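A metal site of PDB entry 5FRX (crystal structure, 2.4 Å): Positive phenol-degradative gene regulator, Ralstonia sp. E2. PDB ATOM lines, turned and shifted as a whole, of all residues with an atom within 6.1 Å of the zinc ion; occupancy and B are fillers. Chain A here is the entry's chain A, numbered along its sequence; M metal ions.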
ATOM      1  N   TRP A 130     -28.277   9.338   0.845  1.00  0.00           N
ATOM      2  CA  TRP A 130     -27.582  10.628   1.051  1.00  0.00           C
ATOM      3  C   TRP A 130     -26.295  10.708   0.241  1.00  0.00           C
ATOM      4  O   TRP A 130     -25.320  10.051   0.559  1.00  0.00           O
ATOM      5  CB  TRP A 130     -27.218  10.829   2.535  1.00  0.00           C
ATOM      6  CG  TRP A 130     -28.299  11.423   3.401  1.00  0.00           C
ATOM      7  CD1 TRP A 130     -29.425  12.071   2.994  1.00  0.00           C
ATOM      8  CD2 TRP A 130     -28.353  11.399   4.841  1.00  0.00           C
ATOM      9  NE1 TRP A 130     -30.175  12.453   4.092  1.00  0.00           N
ATOM     10  CE2 TRP A 130     -29.536  12.043   5.237  1.00  0.00           C
ATOM     11  CE3 TRP A 130     -27.506  10.883   5.837  1.00  0.00           C
ATOM     12  CZ2 TRP A 130     -29.904  12.202   6.570  1.00  0.00           C
ATOM     13  CZ3 TRP A 130     -27.880  11.029   7.172  1.00  0.00           C
ATOM     14  CH2 TRP A 130     -29.058  11.687   7.520  1.00  0.00           C
ATOM     15  N   SER A 133     -22.530  13.841   1.642  1.00  0.00           N
ATOM     16  CA  SER A 133     -22.808  14.323   2.980  1.00  0.00           C
ATOM     17  C   SER A 133     -21.723  15.252   3.386  1.00  0.00           C
ATOM     18  O   SER A 133     -20.596  14.859   3.431  1.00  0.00           O
ATOM     19  CB  SER A 133     -22.827  13.181   3.962  1.00  0.00           C
ATOM     20  OG  SER A 133     -24.091  12.612   4.085  1.00  0.00           O
ATOM     21  N   GLY A 136     -20.220  13.712   6.819  1.00  0.00           N
ATOM     22  CA  GLY A 136     -19.308  12.596   6.667  1.00  0.00           C
ATOM     23  C   GLY A 136     -17.958  13.099   6.147  1.00  0.00           C
ATOM     24  O   GLY A 136     -16.923  12.861   6.769  1.00  0.00           O
ATOM     25  N   PRO A 149     -21.362   5.584  12.063  1.00  0.00           N
ATOM     26  CA  PRO A 149     -21.902   6.744  11.316  1.00  0.00           C
ATOM     27  C   PRO A 149     -21.712   8.084  12.034  1.00  0.00           C
ATOM     28  O   PRO A 149     -21.804   8.150  13.264  1.00  0.00           O
ATOM     29  CB  PRO A 149     -23.393   6.413  11.195  1.00  0.00           C
ATOM     30  CG  PRO A 149     -23.430   4.930  11.137  1.00  0.00           C
ATOM     31  CD  PRO A 149     -22.325   4.469  12.096  1.00  0.00           C
ATOM     32  N   VAL A 150     -21.460   9.139  11.253  1.00  0.00           N
ATOM     33  CA  VAL A 150     -20.995  10.424  11.803  1.00  0.00           C
ATOM     34  C   VAL A 150     -21.904  11.629  11.465  1.00  0.00           C
ATOM     35  O   VAL A 150     -21.759  12.708  12.056  1.00  0.00           O
ATOM     36  CB  VAL A 150     -19.538  10.731  11.310  1.00  0.00           C
ATOM     37  CG1 VAL A 150     -18.546   9.869  12.057  1.00  0.00           C
ATOM     38  CG2 VAL A 150     -19.407  10.468   9.821  1.00  0.00           C
ATOM     39  N   CYS A 151     -22.836  11.435  10.524  1.00  0.00           N
ATOM     40  CA  CYS A 151     -23.788  12.481  10.153  1.00  0.00           C
ATOM     41  C   CYS A 151     -24.840  12.735  11.246  1.00  0.00           C
ATOM     42  O   CYS A 151     -26.047  12.546  11.062  1.00  0.00           O
ATOM     43  CB  CYS A 151     -24.427  12.107   8.817  1.00  0.00           C
ATOM     44  SG  CYS A 151     -23.144  11.770   7.543  1.00  0.00           S
ATOM     45  N   GLN A 154     -27.056  15.791  10.519  1.00  0.00           N
ATOM     46  CA  GLN A 154     -27.931  15.468   9.398  1.00  0.00           C
ATOM     47  C   GLN A 154     -29.047  14.515   9.811  1.00  0.00           C
ATOM     48  O   GLN A 154     -30.158  14.611   9.307  1.00  0.00           O
ATOM     49  CB  GLN A 154     -27.131  14.854   8.262  1.00  0.00           C
ATOM     50  CG  GLN A 154     -26.021  15.763   7.765  1.00  0.00           C
ATOM     51  CD  GLN A 154     -25.217  15.134   6.647  1.00  0.00           C
ATOM     52  OE1 GLN A 154     -24.201  15.687   6.225  1.00  0.00           O
ATOM     53  NE2 GLN A 154     -25.660  13.985   6.161  1.00  0.00           N
ATOM     54  N   GLU A 174     -28.685   6.076  10.564  1.00  0.00           N
ATOM     55  CA  GLU A 174     -27.872   5.816   9.376  1.00  0.00           C
ATOM     56  C   GLU A 174     -27.573   4.331   9.320  1.00  0.00           C
ATOM     57  O   GLU A 174     -27.017   3.778  10.260  1.00  0.00           O
ATOM     58  CB  GLU A 174     -26.557   6.608   9.408  1.00  0.00           C
ATOM     59  CG  GLU A 174     -26.670   8.104   9.217  1.00  0.00           C
ATOM     60  CD  GLU A 174     -25.317   8.755   8.937  1.00  0.00           C
ATOM     61  OE1 GLU A 174     -24.870   8.750   7.766  1.00  0.00           O
ATOM     62  OE2 GLU A 174     -24.699   9.257   9.895  1.00  0.00           O
ATOM     63  N   GLU A 176     -25.848   2.936   6.543  1.00  0.00           N
ATOM     64  CA  GLU A 176     -24.506   2.971   5.986  1.00  0.00           C
ATOM     65  C   GLU A 176     -24.054   4.429   5.915  1.00  0.00           C
ATOM     66  O   GLU A 176     -24.887   5.328   5.757  1.00  0.00           O
ATOM     67  CB  GLU A 176     -24.470   2.314   4.590  1.00  0.00           C
ATOM     68  CG  GLU A 176     -25.340   1.053   4.454  1.00  0.00           C
ATOM     69  CD  GLU A 176     -24.598  -0.247   4.819  1.00  0.00           C
ATOM     70  OE1 GLU A 176     -23.481  -0.177   5.378  1.00  0.00           O
ATOM     71  OE2 GLU A 176     -25.138  -1.333   4.527  1.00  0.00           O
ATOM     72  N   CYS A 177     -22.758   4.671   6.055  1.00  0.00           N
ATOM     73  CA  CYS A 177     -22.274   6.040   6.186  1.00  0.00           C
ATOM     74  C   CYS A 177     -20.930   6.261   5.490  1.00  0.00           C
ATOM     75  O   CYS A 177     -19.989   5.478   5.659  1.00  0.00           O
ATOM     76  CB  CYS A 177     -22.187   6.415   7.669  1.00  0.00           C
ATOM     77  SG  CYS A 177     -21.542   8.089   8.016  1.00  0.00           S
ATOM     78  N   VAL A 178     -20.831   7.350   4.733  1.00  0.00           N
ATOM     79  CA  VAL A 178     -19.577   7.715   4.099  1.00  0.00           C
ATOM     80  C   VAL A 178     -18.455   7.864   5.121  1.00  0.00           C
ATOM     81  O   VAL A 178     -17.283   7.695   4.798  1.00  0.00           O
ATOM     82  CB  VAL A 178     -19.709   9.014   3.319  1.00  0.00           C
ATOM     83  CG1 VAL A 178     -20.921   8.952   2.409  1.00  0.00           C
ATOM     84  CG2 VAL A 178     -19.819  10.202   4.285  1.00  0.00           C
ATOM     85  N   GLY A 179     -18.828   8.186   6.352  1.00  0.00           N
ATOM     86  CA  GLY A 179     -17.834   8.379   7.385  1.00  0.00           C
ATOM     87  C   GLY A 179     -17.136   7.088   7.718  1.00  0.00           C
ATOM     88  O   GLY A 179     -16.020   7.096   8.233  1.00  0.00           O
ATOM     89  N   HIS A 184     -21.668   5.965   0.281  1.00  0.00           N
ATOM     90  CA  HIS A 184     -22.666   6.985   0.563  1.00  0.00           C
ATOM     91  C   HIS A 184     -23.185   6.798   1.960  1.00  0.00           C
ATOM     92  O   HIS A 184     -22.638   5.983   2.728  1.00  0.00           O
ATOM     93  CB  HIS A 184     -23.801   6.916  -0.452  1.00  0.00           C
ATOM     94  CG  HIS A 184     -24.302   5.525  -0.716  1.00  0.00           C
ATOM     95  ND1 HIS A 184     -24.096   4.885  -1.917  1.00  0.00           N
ATOM     96  CD2 HIS A 184     -24.990   4.662   0.066  1.00  0.00           C
ATOM     97  CE1 HIS A 184     -24.639   3.673  -1.852  1.00  0.00           C
ATOM     98  NE2 HIS A 184     -25.186   3.515  -0.668  1.00  0.00           N
ATOM     99  N   CYS A 185     -24.223   7.547   2.320  1.00  0.00           N
ATOM    100  CA  CYS A 185     -24.957   7.283   3.552  1.00  0.00           C
ATOM    101  C   CYS A 185     -26.326   6.752   3.169  1.00  0.00           C
ATOM    102  O   CYS A 185     -26.778   6.942   2.048  1.00  0.00           O
ATOM    103  CB  CYS A 185     -25.096   8.553   4.429  1.00  0.00           C
ATOM    104  SG  CYS A 185     -23.545   9.445   4.792  1.00  0.00           S
ATOM    105  N   ARG A 186     -26.975   6.078   4.107  1.00  0.00           N
ATOM    106  CA  ARG A 186     -28.270   5.492   3.871  1.00  0.00           C
ATOM    107  C   ARG A 186     -28.985   5.523   5.203  1.00  0.00           C
ATOM    108  O   ARG A 186     -28.384   5.210   6.231  1.00  0.00           O
ATOM    109  CB  ARG A 186     -28.144   4.080   3.320  1.00  0.00           C
ATOM    110  CG  ARG A 186     -29.444   3.395   2.898  1.00  0.00           C
ATOM    111  CD  ARG A 186     -29.165   1.946   2.451  1.00  0.00           C
ATOM    112  NE  ARG A 186     -28.098   1.883   1.446  1.00  0.00           N
ATOM    113  CZ  ARG A 186     -27.262   0.859   1.281  1.00  0.00           C
ATOM    114  NH1 ARG A 186     -27.342  -0.211   2.063  1.00  0.00           N
ATOM    115  NH2 ARG A 186     -26.327   0.921   0.335  1.00  0.00           N
HETATM  116 ZN    ZN M   1     -23.289   9.529   6.952  1.00  0.00          ZN
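Val 178 touches the zinc ion. Within 4 Å of the zinc ion: Cys 151, Glu 174, Cys 177, Val 178 and Cys 185. The nearest printed residue that does not touch the zinc ion is Ser 133 (4.3 Å).
The zinc ion is bound by the side-chain carboxylate (OE1) of Glu 174, at 1.9 Å. The zinc ion is bound by SG of Cys 185 (2.2 Å). The zinc ion is bound by the side-chain sulfur (SG) of Cys 151, at 2.3 Å. The zinc ion is bound by SG of Cys 177 (2.5 Å). The zinc ion has four donor atoms within binding distance.
N of Trp 130 is in hydrogen-bond range of O of Cys 185 (3.1 Å). SG of Cys 151 lies close to OG of Ser 133 (3.7 Å). The side-chain sulfur (SG) of Cys 177 lies close to the backbone NH (N) of Val 150, 3.4 Å away. The side-chain sulfur (SG) of Cys 151 sits close to the side-chain amide nitrogen (NE2) of Gln 154, 3.6 Å away. The backbone NH of Val 178 sits at hydrogen-bond distance from the backbone carbonyl oxygen of His 184 (3.0 Å). The backbone NH (N) of Gly 179 sits close to the side-chain sulfur (SG) of Cys 177 (3.2 Å). SG of Cys 151 lies close to N of Gly 136. The backbone NH (N) of Val 178 lies close to the side-chain sulfur (SG) of Cys 185 (3.4 Å).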
